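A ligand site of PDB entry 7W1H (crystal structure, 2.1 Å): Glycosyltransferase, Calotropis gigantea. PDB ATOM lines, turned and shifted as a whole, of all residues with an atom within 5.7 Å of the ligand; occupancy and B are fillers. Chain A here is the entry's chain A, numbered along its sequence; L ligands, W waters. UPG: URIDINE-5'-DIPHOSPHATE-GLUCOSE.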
ATOM      1  N   LYS A  25      -4.744 -22.298 -22.903  1.00  0.00           N
ATOM      2  CA  LYS A  25      -3.449 -21.768 -23.330  1.00  0.00           C
ATOM      3  C   LYS A  25      -2.309 -22.313 -22.480  1.00  0.00           C
ATOM      4  O   LYS A  25      -1.210 -22.539 -23.004  1.00  0.00           O
ATOM      5  CB  LYS A  25      -3.466 -20.241 -23.268  1.00  0.00           C
ATOM      6  CG  LYS A  25      -4.438 -19.594 -24.252  1.00  0.00           C
ATOM      7  CD  LYS A  25      -3.881 -18.289 -24.768  1.00  0.00           C
ATOM      8  CE  LYS A  25      -4.606 -17.838 -26.021  1.00  0.00           C
ATOM      9  NZ  LYS A  25      -6.034 -17.609 -25.708  1.00  0.00           N
ATOM     10  N   GLY A  26      -2.542 -22.493 -21.176  1.00  0.00           N
ATOM     11  CA  GLY A  26      -1.546 -23.088 -20.301  1.00  0.00           C
ATOM     12  C   GLY A  26      -1.271 -24.553 -20.580  1.00  0.00           C
ATOM     13  O   GLY A  26      -0.269 -25.090 -20.081  1.00  0.00           O
ATOM     14  N   HIS A  27      -2.115 -25.206 -21.357  1.00  0.00           N
ATOM     15  CA  HIS A  27      -1.833 -26.557 -21.846  1.00  0.00           C
ATOM     16  C   HIS A  27      -1.402 -26.568 -23.309  1.00  0.00           C
ATOM     17  O   HIS A  27      -0.514 -27.360 -23.673  1.00  0.00           O
ATOM     18  CB  HIS A  27      -3.060 -27.452 -21.650  1.00  0.00           C
ATOM     19  CG  HIS A  27      -3.488 -27.578 -20.213  1.00  0.00           C
ATOM     20  ND1 HIS A  27      -3.331 -28.738 -19.490  1.00  0.00           N
ATOM     21  CD2 HIS A  27      -4.036 -26.675 -19.361  1.00  0.00           C
ATOM     22  CE1 HIS A  27      -3.771 -28.547 -18.259  1.00  0.00           C
ATOM     23  NE2 HIS A  27      -4.205 -27.310 -18.146  1.00  0.00           N
ATOM     24  N   ASN A  29       0.244 -24.054 -24.986  1.00  0.00           N
ATOM     25  CA  ASN A  29       1.560 -23.451 -25.206  1.00  0.00           C
ATOM     26  C   ASN A  29       2.724 -24.398 -24.918  1.00  0.00           C
ATOM     27  O   ASN A  29       3.674 -24.451 -25.737  1.00  0.00           O
ATOM     28  CB  ASN A  29       1.703 -22.179 -24.370  1.00  0.00           C
ATOM     29  CG  ASN A  29       0.913 -21.007 -24.915  1.00  0.00           C
ATOM     30  OD1 ASN A  29       0.336 -21.077 -26.016  1.00  0.00           O
ATOM     31  ND2 ASN A  29       0.868 -19.919 -24.138  1.00  0.00           N
ATOM     32  N   PRO A  30       2.770 -25.107 -23.777  1.00  0.00           N
ATOM     33  CA  PRO A  30       3.920 -25.998 -23.552  1.00  0.00           C
ATOM     34  C   PRO A  30       3.950 -27.148 -24.529  1.00  0.00           C
ATOM     35  O   PRO A  30       5.046 -27.603 -24.891  1.00  0.00           O
ATOM     36  CB  PRO A  30       3.722 -26.476 -22.101  1.00  0.00           C
ATOM     37  CG  PRO A  30       2.236 -26.323 -21.867  1.00  0.00           C
ATOM     38  CD  PRO A  30       1.878 -25.054 -22.607  1.00  0.00           C
ATOM     39  N   THR A 144       1.687 -30.692 -17.465  1.00  0.00           N
ATOM     40  CA  THR A 144       1.919 -29.257 -17.653  1.00  0.00           C
ATOM     41  C   THR A 144       2.061 -28.518 -16.321  1.00  0.00           C
ATOM     42  O   THR A 144       2.001 -27.289 -16.311  1.00  0.00           O
ATOM     43  CB  THR A 144       0.785 -28.644 -18.489  1.00  0.00           C
ATOM     44  OG1 THR A 144      -0.467 -28.893 -17.845  1.00  0.00           O
ATOM     45  CG2 THR A 144       0.752 -29.264 -19.885  1.00  0.00           C
ATOM     46  N   GLN A 145       2.217 -29.243 -15.216  1.00  0.00           N
ATOM     47  CA  GLN A 145       2.442 -28.661 -13.904  1.00  0.00           C
ATOM     48  C   GLN A 145       3.701 -29.284 -13.306  1.00  0.00           C
ATOM     49  O   GLN A 145       4.155 -30.329 -13.775  1.00  0.00           O
ATOM     50  CB  GLN A 145       1.218 -28.887 -12.994  1.00  0.00           C
ATOM     51  CG  GLN A 145       0.054 -27.947 -13.314  1.00  0.00           C
ATOM     52  CD  GLN A 145      -1.267 -28.429 -12.735  1.00  0.00           C
ATOM     53  OE1 GLN A 145      -1.413 -28.526 -11.506  1.00  0.00           O
ATOM     54  N   GLU A 261       3.031 -14.346 -30.583  1.00  0.00           N
ATOM     55  CA  GLU A 261       1.843 -13.940 -29.858  1.00  0.00           C
ATOM     56  C   GLU A 261       1.270 -12.645 -30.423  1.00  0.00           C
ATOM     57  O   GLU A 261       1.937 -11.897 -31.150  1.00  0.00           O
ATOM     58  CB  GLU A 261       2.134 -13.748 -28.361  1.00  0.00           C
ATOM     59  CG  GLU A 261       2.197 -15.012 -27.510  1.00  0.00           C
ATOM     60  CD  GLU A 261       0.845 -15.676 -27.337  1.00  0.00           C
ATOM     61  OE1 GLU A 261      -0.160 -15.069 -27.736  1.00  0.00           O
ATOM     62  OE2 GLU A 261       0.807 -16.801 -26.788  1.00  0.00           O
ATOM     63  N   TYR A 281       5.719  -6.047 -14.808  1.00  0.00           N
ATOM     64  CA  TYR A 281       4.833  -6.777 -15.715  1.00  0.00           C
ATOM     65  C   TYR A 281       3.792  -7.516 -14.886  1.00  0.00           C
ATOM     66  O   TYR A 281       4.138  -8.241 -13.951  1.00  0.00           O
ATOM     67  CB  TYR A 281       5.609  -7.767 -16.587  1.00  0.00           C
ATOM     68  CG  TYR A 281       4.740  -8.705 -17.405  1.00  0.00           C
ATOM     69  CD1 TYR A 281       3.771  -8.216 -18.258  1.00  0.00           C
ATOM     70  CD2 TYR A 281       4.904 -10.086 -17.321  1.00  0.00           C
ATOM     71  CE1 TYR A 281       2.969  -9.075 -19.008  1.00  0.00           C
ATOM     72  CE2 TYR A 281       4.116 -10.957 -18.063  1.00  0.00           C
ATOM     73  CZ  TYR A 281       3.152 -10.444 -18.914  1.00  0.00           C
ATOM     74  OH  TYR A 281       2.361 -11.310 -19.647  1.00  0.00           O
ATOM     75  N   SER A 283       0.356  -9.944 -15.005  1.00  0.00           N
ATOM     76  CA  SER A 283      -0.550 -10.812 -15.740  1.00  0.00           C
ATOM     77  C   SER A 283      -1.110 -11.887 -14.814  1.00  0.00           C
ATOM     78  O   SER A 283      -0.382 -12.479 -14.013  1.00  0.00           O
ATOM     79  CB  SER A 283       0.143 -11.461 -16.948  1.00  0.00           C
ATOM     80  OG  SER A 283      -0.745 -12.331 -17.622  1.00  0.00           O
ATOM     81  N   PHE A 284      -2.415 -12.142 -14.934  1.00  0.00           N
ATOM     82  CA  PHE A 284      -3.065 -13.191 -14.153  1.00  0.00           C
ATOM     83  C   PHE A 284      -3.460 -14.373 -15.043  1.00  0.00           C
ATOM     84  O   PHE A 284      -4.349 -15.164 -14.695  1.00  0.00           O
ATOM     85  CB  PHE A 284      -4.255 -12.617 -13.384  1.00  0.00           C
ATOM     86  CG  PHE A 284      -3.831 -11.742 -12.232  1.00  0.00           C
ATOM     87  CD1 PHE A 284      -3.392 -10.448 -12.454  1.00  0.00           C
ATOM     88  CD2 PHE A 284      -3.808 -12.249 -10.943  1.00  0.00           C
ATOM     89  CE1 PHE A 284      -2.958  -9.650 -11.399  1.00  0.00           C
ATOM     90  CE2 PHE A 284      -3.383 -11.453  -9.877  1.00  0.00           C
ATOM     91  CZ  PHE A 284      -2.956 -10.152 -10.117  1.00  0.00           C
ATOM     92  N   GLY A 285      -2.762 -14.534 -16.162  1.00  0.00           N
ATOM     93  CA  GLY A 285      -2.941 -15.703 -17.009  1.00  0.00           C
ATOM     94  C   GLY A 285      -4.176 -15.597 -17.879  1.00  0.00           C
ATOM     95  O   GLY A 285      -4.769 -14.532 -18.070  1.00  0.00           O
ATOM     96  N   SER A 286      -4.574 -16.757 -18.408  1.00  0.00           N
ATOM     97  CA  SER A 286      -5.599 -16.786 -19.449  1.00  0.00           C
ATOM     98  C   SER A 286      -6.984 -17.147 -18.930  1.00  0.00           C
ATOM     99  O   SER A 286      -7.949 -17.038 -19.695  1.00  0.00           O
ATOM    100  CB  SER A 286      -5.191 -17.769 -20.554  1.00  0.00           C
ATOM    101  OG  SER A 286      -5.206 -19.103 -20.070  1.00  0.00           O
ATOM    102  N   ILE A 287      -7.119 -17.533 -17.665  1.00  0.00           N
ATOM    103  CA  ILE A 287      -8.377 -18.091 -17.149  1.00  0.00           C
ATOM    104  C   ILE A 287      -8.838 -17.324 -15.922  1.00  0.00           C
ATOM    105  O   ILE A 287     -10.039 -17.033 -15.778  1.00  0.00           O
ATOM    106  CB  ILE A 287      -8.216 -19.595 -16.828  1.00  0.00           C
ATOM    107  CG1 ILE A 287      -7.607 -20.327 -18.016  1.00  0.00           C
ATOM    108  CG2 ILE A 287      -9.549 -20.201 -16.397  1.00  0.00           C
ATOM    109  CD1 ILE A 287      -8.565 -20.534 -19.173  1.00  0.00           C
ATOM    110  N   ALA A 288      -7.917 -17.023 -14.998  1.00  0.00           N
ATOM    111  CA  ALA A 288      -8.306 -16.393 -13.746  1.00  0.00           C
ATOM    112  C   ALA A 288      -9.066 -15.096 -14.005  1.00  0.00           C
ATOM    113  O   ALA A 288      -8.801 -14.368 -14.972  1.00  0.00           O
ATOM    114  CB  ALA A 288      -7.077 -16.123 -12.873  1.00  0.00           C
ATOM    115  N   VAL A 312      -1.656  -6.865 -18.327  1.00  0.00           N
ATOM    116  CA  VAL A 312      -2.491  -7.599 -19.278  1.00  0.00           C
ATOM    117  C   VAL A 312      -3.866  -7.730 -18.649  1.00  0.00           C
ATOM    118  O   VAL A 312      -4.033  -8.398 -17.621  1.00  0.00           O
ATOM    119  CB  VAL A 312      -1.889  -8.969 -19.607  1.00  0.00           C
ATOM    120  CG1 VAL A 312      -2.917  -9.820 -20.355  1.00  0.00           C
ATOM    121  CG2 VAL A 312      -0.607  -8.825 -20.442  1.00  0.00           C
ATOM    122  N   ASN A 352      -4.732  -6.154 -23.928  1.00  0.00           N
ATOM    123  CA  ASN A 352      -5.552  -7.343 -23.762  1.00  0.00           C
ATOM    124  C   ASN A 352      -4.756  -8.647 -23.852  1.00  0.00           C
ATOM    125  O   ASN A 352      -5.279  -9.687 -23.452  1.00  0.00           O
ATOM    126  CB  ASN A 352      -6.700  -7.344 -24.777  1.00  0.00           C
ATOM    127  CG  ASN A 352      -6.248  -7.729 -26.173  1.00  0.00           C
ATOM    128  OD1 ASN A 352      -5.328  -7.124 -26.754  1.00  0.00           O
ATOM    129  N   TRP A 353      -3.512  -8.602 -24.313  1.00  0.00           N
ATOM    130  CA  TRP A 353      -2.645  -9.763 -24.465  1.00  0.00           C
ATOM    131  C   TRP A 353      -1.282  -9.266 -24.928  1.00  0.00           C
ATOM    132  O   TRP A 353      -1.169  -8.173 -25.480  1.00  0.00           O
ATOM    133  CB  TRP A 353      -3.190 -10.796 -25.470  1.00  0.00           C
ATOM    134  CG  TRP A 353      -2.712 -12.238 -25.252  1.00  0.00           C
ATOM    135  CD1 TRP A 353      -1.931 -12.988 -26.111  1.00  0.00           C
ATOM    136  CD2 TRP A 353      -3.028 -13.096 -24.146  1.00  0.00           C
ATOM    137  NE1 TRP A 353      -1.730 -14.252 -25.577  1.00  0.00           N
ATOM    138  CE2 TRP A 353      -2.398 -14.343 -24.380  1.00  0.00           C
ATOM    139  CE3 TRP A 353      -3.773 -12.932 -22.972  1.00  0.00           C
ATOM    140  CZ2 TRP A 353      -2.490 -15.402 -23.490  1.00  0.00           C
ATOM    141  CZ3 TRP A 353      -3.870 -14.003 -22.090  1.00  0.00           C
ATOM    142  CH2 TRP A 353      -3.236 -15.219 -22.359  1.00  0.00           C
ATOM    143  N   CYS A 354      -0.259 -10.093 -24.716  1.00  0.00           N
ATOM    144  CA  CYS A 354       1.123  -9.690 -24.963  1.00  0.00           C
ATOM    145  C   CYS A 354       1.942 -10.936 -25.244  1.00  0.00           C
ATOM    146  O   CYS A 354       1.532 -12.051 -24.873  1.00  0.00           O
ATOM    147  CB  CYS A 354       1.691  -8.918 -23.764  1.00  0.00           C
ATOM    148  SG  CYS A 354       2.349  -9.998 -22.435  1.00  0.00           S
ATOM    149  N   PRO A 355       3.096 -10.811 -25.920  1.00  0.00           N
ATOM    150  CA  PRO A 355       3.972 -11.969 -26.082  1.00  0.00           C
ATOM    151  C   PRO A 355       4.735 -12.205 -24.786  1.00  0.00           C
ATOM    152  O   PRO A 355       5.809 -11.620 -24.590  1.00  0.00           O
ATOM    153  CB  PRO A 355       4.881 -11.567 -27.247  1.00  0.00           C
ATOM    154  CG  PRO A 355       4.982 -10.061 -27.149  1.00  0.00           C
ATOM    155  CD  PRO A 355       3.703  -9.580 -26.480  1.00  0.00           C
ATOM    156  N   GLN A 356       4.177 -13.017 -23.880  1.00  0.00           N
ATOM    157  CA  GLN A 356       4.656 -12.982 -22.504  1.00  0.00           C
ATOM    158  C   GLN A 356       6.130 -13.357 -22.412  1.00  0.00           C
ATOM    159  O   GLN A 356       6.891 -12.718 -21.682  1.00  0.00           O
ATOM    160  CB  GLN A 356       3.826 -13.897 -21.601  1.00  0.00           C
ATOM    161  CG  GLN A 356       4.530 -14.180 -20.273  1.00  0.00           C
ATOM    162  CD  GLN A 356       3.587 -14.743 -19.199  1.00  0.00           C
ATOM    163  OE1 GLN A 356       3.805 -15.830 -18.688  1.00  0.00           O
ATOM    164  NE2 GLN A 356       2.569 -13.986 -18.859  1.00  0.00           N
ATOM    165  N   LEU A 357       6.561 -14.362 -23.164  1.00  0.00           N
ATOM    166  CA  LEU A 357       7.954 -14.787 -23.078  1.00  0.00           C
ATOM    167  C   LEU A 357       8.906 -13.682 -23.524  1.00  0.00           C
ATOM    168  O   LEU A 357       9.977 -13.495 -22.929  1.00  0.00           O
ATOM    169  CB  LEU A 357       8.155 -16.055 -23.906  1.00  0.00           C
ATOM    170  CG  LEU A 357       9.463 -16.810 -23.708  1.00  0.00           C
ATOM    171  CD1 LEU A 357       9.737 -17.021 -22.240  1.00  0.00           C
ATOM    172  CD2 LEU A 357       9.370 -18.148 -24.434  1.00  0.00           C
ATOM    173  N   HIS A 371      -0.135 -14.621 -11.280  1.00  0.00           N
ATOM    174  CA  HIS A 371      -1.002 -15.544 -10.561  1.00  0.00           C
ATOM    175  C   HIS A 371      -0.336 -16.893 -10.311  1.00  0.00           C
ATOM    176  O   HIS A 371      -0.964 -17.763  -9.698  1.00  0.00           O
ATOM    177  CB  HIS A 371      -2.306 -15.746 -11.337  1.00  0.00           C
ATOM    178  CG  HIS A 371      -2.197 -16.700 -12.479  1.00  0.00           C
ATOM    179  ND1 HIS A 371      -1.245 -16.568 -13.473  1.00  0.00           N
ATOM    180  CD2 HIS A 371      -2.936 -17.789 -12.802  1.00  0.00           C
ATOM    181  CE1 HIS A 371      -1.399 -17.544 -14.359  1.00  0.00           C
ATOM    182  NE2 HIS A 371      -2.420 -18.298 -13.980  1.00  0.00           N
ATOM    183  N   CYS A 372       0.907 -17.076 -10.777  1.00  0.00           N
ATOM    184  CA  CYS A 372       1.715 -18.256 -10.484  1.00  0.00           C
ATOM    185  C   CYS A 372       1.211 -19.508 -11.174  1.00  0.00           C
ATOM    186  O   CYS A 372       1.442 -20.614 -10.685  1.00  0.00           O
ATOM    187  CB  CYS A 372       1.813 -18.513  -8.979  1.00  0.00           C
ATOM    188  SG  CYS A 372       2.510 -17.134  -8.101  1.00  0.00           S
ATOM    189  N   GLY A 373       0.513 -19.382 -12.304  1.00  0.00           N
ATOM    190  CA  GLY A 373       0.388 -20.526 -13.184  1.00  0.00           C
ATOM    191  C   GLY A 373       1.746 -21.125 -13.487  1.00  0.00           C
ATOM    192  O   GLY A 373       2.773 -20.445 -13.391  1.00  0.00           O
ATOM    193  N   TRP A 374       1.777 -22.429 -13.807  1.00  0.00           N
ATOM    194  CA  TRP A 374       3.086 -23.068 -13.944  1.00  0.00           C
ATOM    195  C   TRP A 374       3.850 -22.549 -15.162  1.00  0.00           C
ATOM    196  O   TRP A 374       5.057 -22.349 -15.072  1.00  0.00           O
ATOM    197  CB  TRP A 374       3.009 -24.601 -14.002  1.00  0.00           C
ATOM    198  CG  TRP A 374       4.407 -25.234 -14.111  1.00  0.00           C
ATOM    199  CD1 TRP A 374       4.858 -26.060 -15.099  1.00  0.00           C
ATOM    200  CD2 TRP A 374       5.530 -25.052 -13.209  1.00  0.00           C
ATOM    201  NE1 TRP A 374       6.182 -26.399 -14.877  1.00  0.00           N
ATOM    202  CE2 TRP A 374       6.615 -25.789 -13.724  1.00  0.00           C
ATOM    203  CE3 TRP A 374       5.715 -24.331 -12.017  1.00  0.00           C
ATOM    204  CZ2 TRP A 374       7.866 -25.841 -13.089  1.00  0.00           C
ATOM    205  CZ3 TRP A 374       6.959 -24.364 -11.392  1.00  0.00           C
ATOM    206  CH2 TRP A 374       8.015 -25.123 -11.937  1.00  0.00           C
ATOM    207  N   ASN A 375       3.175 -22.331 -16.295  1.00  0.00           N
ATOM    208  CA  ASN A 375       3.934 -21.819 -17.443  1.00  0.00           C
ATOM    209  C   ASN A 375       4.487 -20.434 -17.119  1.00  0.00           C
ATOM    210  O   ASN A 375       5.674 -20.163 -17.348  1.00  0.00           O
ATOM    211  CB  ASN A 375       3.068 -21.789 -18.712  1.00  0.00           C
ATOM    212  CG  ASN A 375       2.605 -23.172 -19.130  1.00  0.00           C
ATOM    213  OD1 ASN A 375       3.343 -23.918 -19.797  1.00  0.00           O
ATOM    214  ND2 ASN A 375       1.384 -23.537 -18.718  1.00  0.00           N
ATOM    215  N   SER A 376       3.658 -19.561 -16.531  1.00  0.00           N
ATOM    216  CA  SER A 376       4.146 -18.236 -16.137  1.00  0.00           C
ATOM    217  C   SER A 376       5.339 -18.354 -15.193  1.00  0.00           C
ATOM    218  O   SER A 376       6.375 -17.716 -15.402  1.00  0.00           O
ATOM    219  CB  SER A 376       3.024 -17.431 -15.494  1.00  0.00           C
ATOM    220  OG  SER A 376       2.094 -17.059 -16.498  1.00  0.00           O
ATOM    221  N   THR A 377       5.216 -19.193 -14.165  1.00  0.00           N
ATOM    222  CA  THR A 377       6.291 -19.405 -13.203  1.00  0.00           C
ATOM    223  C   THR A 377       7.557 -19.878 -13.889  1.00  0.00           C
ATOM    224  O   THR A 377       8.640 -19.316 -13.692  1.00  0.00           O
ATOM    225  CB  THR A 377       5.841 -20.423 -12.121  1.00  0.00           C
ATOM    226  OG1 THR A 377       4.638 -19.980 -11.484  1.00  0.00           O
ATOM    227  CG2 THR A 377       6.906 -20.616 -11.069  1.00  0.00           C
ATOM    228  N   GLU A 379       8.315 -19.814 -17.115  1.00  0.00           N
ATOM    229  CA  GLU A 379       8.826 -18.844 -18.083  1.00  0.00           C
ATOM    230  C   GLU A 379       9.616 -17.742 -17.381  1.00  0.00           C
ATOM    231  O   GLU A 379      10.638 -17.291 -17.890  1.00  0.00           O
ATOM    232  CB  GLU A 379       7.683 -18.246 -18.902  1.00  0.00           C
ATOM    233  CG  GLU A 379       7.099 -19.216 -19.923  1.00  0.00           C
ATOM    234  CD  GLU A 379       5.705 -18.822 -20.377  1.00  0.00           C
ATOM    235  OE1 GLU A 379       5.276 -17.684 -20.126  1.00  0.00           O
ATOM    236  OE2 GLU A 379       5.027 -19.659 -20.996  1.00  0.00           O
ATOM    237  N   TRP A 393      -5.849 -20.308  -7.670  1.00  0.00           N
ATOM    238  CA  TRP A 393      -6.369 -21.630  -7.306  1.00  0.00           C
ATOM    239  C   TRP A 393      -5.557 -22.734  -7.970  1.00  0.00           C
ATOM    240  O   TRP A 393      -4.580 -22.489  -8.686  1.00  0.00           O
ATOM    241  CB  TRP A 393      -7.861 -21.744  -7.659  1.00  0.00           C
ATOM    242  CG  TRP A 393      -8.257 -20.880  -8.816  1.00  0.00           C
ATOM    243  CD1 TRP A 393      -9.016 -19.740  -8.776  1.00  0.00           C
ATOM    244  CD2 TRP A 393      -7.925 -21.088 -10.198  1.00  0.00           C
ATOM    245  NE1 TRP A 393      -9.164 -19.221 -10.054  1.00  0.00           N
ATOM    246  CE2 TRP A 393      -8.497 -20.035 -10.931  1.00  0.00           C
ATOM    247  CE3 TRP A 393      -7.180 -22.057 -10.873  1.00  0.00           C
ATOM    248  CZ2 TRP A 393      -8.366 -19.930 -12.313  1.00  0.00           C
ATOM    249  CZ3 TRP A 393      -7.037 -21.947 -12.243  1.00  0.00           C
ATOM    250  CH2 TRP A 393      -7.628 -20.895 -12.947  1.00  0.00           C
ATOM    251  N   VAL A 394      -5.988 -23.989  -7.731  1.00  0.00           N
ATOM    252  CA  VAL A 394      -5.284 -25.196  -8.146  1.00  0.00           C
ATOM    253  C   VAL A 394      -3.802 -25.073  -7.789  1.00  0.00           C
ATOM    254  O   VAL A 394      -3.464 -24.756  -6.644  1.00  0.00           O
ATOM    255  CB  VAL A 394      -5.538 -25.479  -9.637  1.00  0.00           C
ATOM    256  CG1 VAL A 394      -5.078 -26.889 -10.002  1.00  0.00           C
ATOM    257  CG2 VAL A 394      -7.041 -25.390  -9.907  1.00  0.00           C
ATOM    258  N   ASP A 395      -2.901 -25.312  -8.758  1.00  0.00           N
ATOM    259  CA  ASP A 395      -1.488 -25.424  -8.419  1.00  0.00           C
ATOM    260  C   ASP A 395      -0.834 -24.089  -8.071  1.00  0.00           C
ATOM    261  O   ASP A 395       0.305 -24.100  -7.549  1.00  0.00           O
ATOM    262  CB  ASP A 395      -0.704 -26.089  -9.565  1.00  0.00           C
ATOM    263  CG  ASP A 395      -0.808 -25.327 -10.890  1.00  0.00           C
ATOM    264  OD1 ASP A 395      -1.900 -24.814 -11.207  1.00  0.00           O
ATOM    265  OD2 ASP A 395       0.194 -25.278 -11.609  1.00  0.00           O
ATOM    266  N   GLN A 396      -1.498 -22.963  -8.296  1.00  0.00           N
ATOM    267  CA  GLN A 396      -0.838 -21.662  -8.122  1.00  0.00           C
ATOM    268  C   GLN A 396      -0.451 -21.404  -6.668  1.00  0.00           C
ATOM    269  O   GLN A 396       0.577 -20.745  -6.416  1.00  0.00           O
ATOM    270  CB  GLN A 396      -1.744 -20.539  -8.637  1.00  0.00           C
ATOM    271  CG  GLN A 396      -2.112 -20.747 -10.099  1.00  0.00           C
ATOM    272  CD  GLN A 396      -3.459 -20.193 -10.460  1.00  0.00           C
ATOM    273  OE1 GLN A 396      -4.023 -19.372  -9.720  1.00  0.00           O
ATOM    274  NE2 GLN A 396      -3.979 -20.592 -11.630  1.00  0.00           N
ATOM    275  N   ASN A 399       2.762 -23.484  -6.142  1.00  0.00           N
ATOM    276  CA  ASN A 399       3.854 -22.860  -6.884  1.00  0.00           C
ATOM    277  C   ASN A 399       4.375 -21.617  -6.163  1.00  0.00           C
ATOM    278  O   ASN A 399       5.589 -21.396  -6.081  1.00  0.00           O
ATOM    279  CB  ASN A 399       3.372 -22.504  -8.308  1.00  0.00           C
ATOM    280  CG  ASN A 399       2.953 -23.730  -9.126  1.00  0.00           C
ATOM    281  OD1 ASN A 399       3.255 -24.877  -8.760  1.00  0.00           O
ATOM    282  ND2 ASN A 399       2.249 -23.490 -10.231  1.00  0.00           N
HETATM  283  N1  UPG L   1       0.440 -15.744 -21.879  1.00  0.00           N
HETATM  284  C2  UPG L   1       0.731 -14.993 -22.996  1.00  0.00           C
HETATM  285  N3  UPG L   1       0.352 -13.680 -22.940  1.00  0.00           N
HETATM  286  C4  UPG L   1      -0.283 -13.040 -21.884  1.00  0.00           C
HETATM  287  C5  UPG L   1      -0.553 -13.883 -20.763  1.00  0.00           C
HETATM  288  C6  UPG L   1      -0.193 -15.185 -20.796  1.00  0.00           C
HETATM  289  O2  UPG L   1       1.301 -15.464 -23.976  1.00  0.00           O
HETATM  290  O4  UPG L   1      -0.551 -11.846 -21.983  1.00  0.00           O
HETATM  291  C1C UPG L   1       0.824 -17.167 -21.905  1.00  0.00           C
HETATM  292  C2C UPG L   1       1.991 -17.489 -20.961  1.00  0.00           C
HETATM  293  O2C UPG L   1       3.202 -17.173 -21.611  1.00  0.00           O
HETATM  294  C3C UPG L   1       1.753 -18.988 -20.711  1.00  0.00           C
HETATM  295  C4C UPG L   1       0.218 -19.058 -20.653  1.00  0.00           C
HETATM  296  O4C UPG L   1      -0.261 -17.961 -21.476  1.00  0.00           O
HETATM  297  O3C UPG L   1       2.258 -19.797 -21.762  1.00  0.00           O
HETATM  298  C5C UPG L   1      -0.386 -18.941 -19.279  1.00  0.00           C
HETATM  299  O5C UPG L   1      -0.288 -20.223 -18.648  1.00  0.00           O
HETATM  300  PA  UPG L   1      -0.177 -20.373 -17.066  1.00  0.00           P
HETATM  301  O1A UPG L   1       0.821 -19.389 -16.533  1.00  0.00           O
HETATM  302  O2A UPG L   1       0.049 -21.812 -16.739  1.00  0.00           O
HETATM  303  O3A UPG L   1      -1.652 -19.973 -16.585  1.00  0.00           O
HETATM  304  PB  UPG L   1      -3.160 -20.434 -16.914  1.00  0.00           P
HETATM  305  O1B UPG L   1      -3.605 -19.695 -18.136  1.00  0.00           O
HETATM  306  O2B UPG L   1      -3.961 -20.132 -15.693  1.00  0.00           O
HETATM  307  O3B UPG L   1      -3.026 -22.044 -17.136  1.00  0.00           O
HETATM  308  C1' UPG L   1      -3.714 -23.153 -16.515  1.00  0.00           C
HETATM  309  C2' UPG L   1      -3.859 -23.007 -14.983  1.00  0.00           C
HETATM  310  C3' UPG L   1      -2.455 -22.969 -14.356  1.00  0.00           C
HETATM  311  C4' UPG L   1      -1.732 -24.266 -14.714  1.00  0.00           C
HETATM  312  C5' UPG L   1      -1.699 -24.397 -16.233  1.00  0.00           C
HETATM  313  C6' UPG L   1      -0.998 -25.650 -16.729  1.00  0.00           C
HETATM  314  O2' UPG L   1      -4.761 -21.974 -14.621  1.00  0.00           O
HETATM  315  O3' UPG L   1      -2.525 -22.783 -12.938  1.00  0.00           O
HETATM  316  O4' UPG L   1      -0.391 -24.223 -14.261  1.00  0.00           O
HETATM  317  O5' UPG L   1      -3.047 -24.381 -16.760  1.00  0.00           O
HETATM  318  O6' UPG L   1      -1.578 -26.869 -16.247  1.00  0.00           O
HETATM  319  O   HOH W   1      -5.387 -17.952 -15.546  1.00  0.00           O
HETATM  320  O   HOH W   2       0.435 -14.885 -17.549  1.00  0.00           O
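An oxygen (O1B) of the ligand is in hydrogen-bond range of the backbone NH (N) of Ser 286 (3.1 Å). OG of Ser 286 sits at hydrogen-bond distance from O1B of the ligand, 2.6 Å away. An oxygen (O2C) of the ligand sits at hydrogen-bond distance from the side-chain carboxylate of Glu 379, at 2.6 Å. An oxygen (O1A) of the ligand sits at hydrogen-bond distance from the backbone NH (N) of Ser 376. OG of Ser 376 lies within hydrogen-bond range of O1A of the ligand, 2.7 Å away. The side-chain carboxylate (OD1) of Asp 395 lies within hydrogen-bond range of an oxygen (O3') of the ligand, at 2.7 Å. An oxygen (O3C) of the ligand lies within hydrogen-bond range of the side-chain amide nitrogen (ND2) of Asn 29 (2.8 Å). The backbone NH (N) of Cys 354 lies within hydrogen-bond range of an oxygen (O4) of the ligand (3.3 Å). O of Cys 354 sits at hydrogen-bond distance from N3 of the ligand (2.8 Å). The side-chain sulfur (SG) of Cys 354 is in hydrogen-bond range of an oxygen (O4) of the ligand (3.5 Å). The side-chain hydroxyl (OG1) of Thr 144 sits at hydrogen-bond distance from an oxygen (O6') of the ligand, at 2.8 Å. An oxygen (O4') of the ligand sits at hydrogen-bond distance from the backbone NH of Trp 374 (2.9 Å). The side-chain amide nitrogen (NE2) of Gln 396 is in hydrogen-bond range of an oxygen (O3') of the ligand. NE2 of His 371 sits at hydrogen-bond distance from O2B of the ligand, 2.9 Å away. N of Asn 375 is in hydrogen-bond range of O2A of the ligand (3.2 Å). O2A of the ligand lies within hydrogen-bond range of ND2 of Asn 375 (2.9 Å). A ring nitrogen (NE2) of His 27 sits at hydrogen-bond distance from an oxygen (O6') of the ligand (3.3 Å). The side-chain amide oxygen (OE1) of Gln 356 lies within hydrogen-bond range of an oxygen (O2C) of the ligand (3.3 Å).
The side-chain carboxylate (OE1) of Glu 379 lies close to the side-chain amide oxygen (OE1) of Gln 356 (2.8 Å). The side-chain hydroxyl of Ser 376 sits at hydrogen-bond distance from the side-chain amide oxygen of Gln 356 (3.0 Å). SG of Cys 354 is in hydrogen-bond range of OH of Tyr 281 (3.1 Å). OG1 of Thr 144 sits at hydrogen-bond distance from ND1 of His 27 (3.3 Å). O of His 371 sits close to OE1 of Gln 396 (3.5 Å). ND2 of Asn 375 sits at hydrogen-bond distance from O of Gly 26 (2.6 Å). NE2 of Gln 356 is in hydrogen-bond range of OH of Tyr 281, at 2.8 Å. OG of Ser 283 lies within hydrogen-bond range of N of Gly 285, 3.3 Å away.
OE2 of Glu 261 sits close to O2 of the ligand (3.2 Å). NE1 of Trp 353 sits close to N3 of the ligand (3.4 Å). Gly 26 touches the ligand. Gln 145 touches the ligand (CG to O6', 3.5 Å). Tyr 281 touches the ligand. Ser 283 touches the ligand. CG2 of Val 312 touches O4 of the ligand, at 3.4 Å. CA of Gly 373 touches O1A of the ligand (3.6 Å). Trp 393 touches the ligand. Of the 35 residues printed, 22 come within 4 Å of the ligand. The nearest printed residue that does not touch the ligand is Ile 287 (4.1 Å).
Water W2 lies within hydrogen-bond range of NE2 of Gln 356 (2.7 Å), OG of Ser 283 (2.8 Å) and OG of Ser 376 (2.9 Å).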
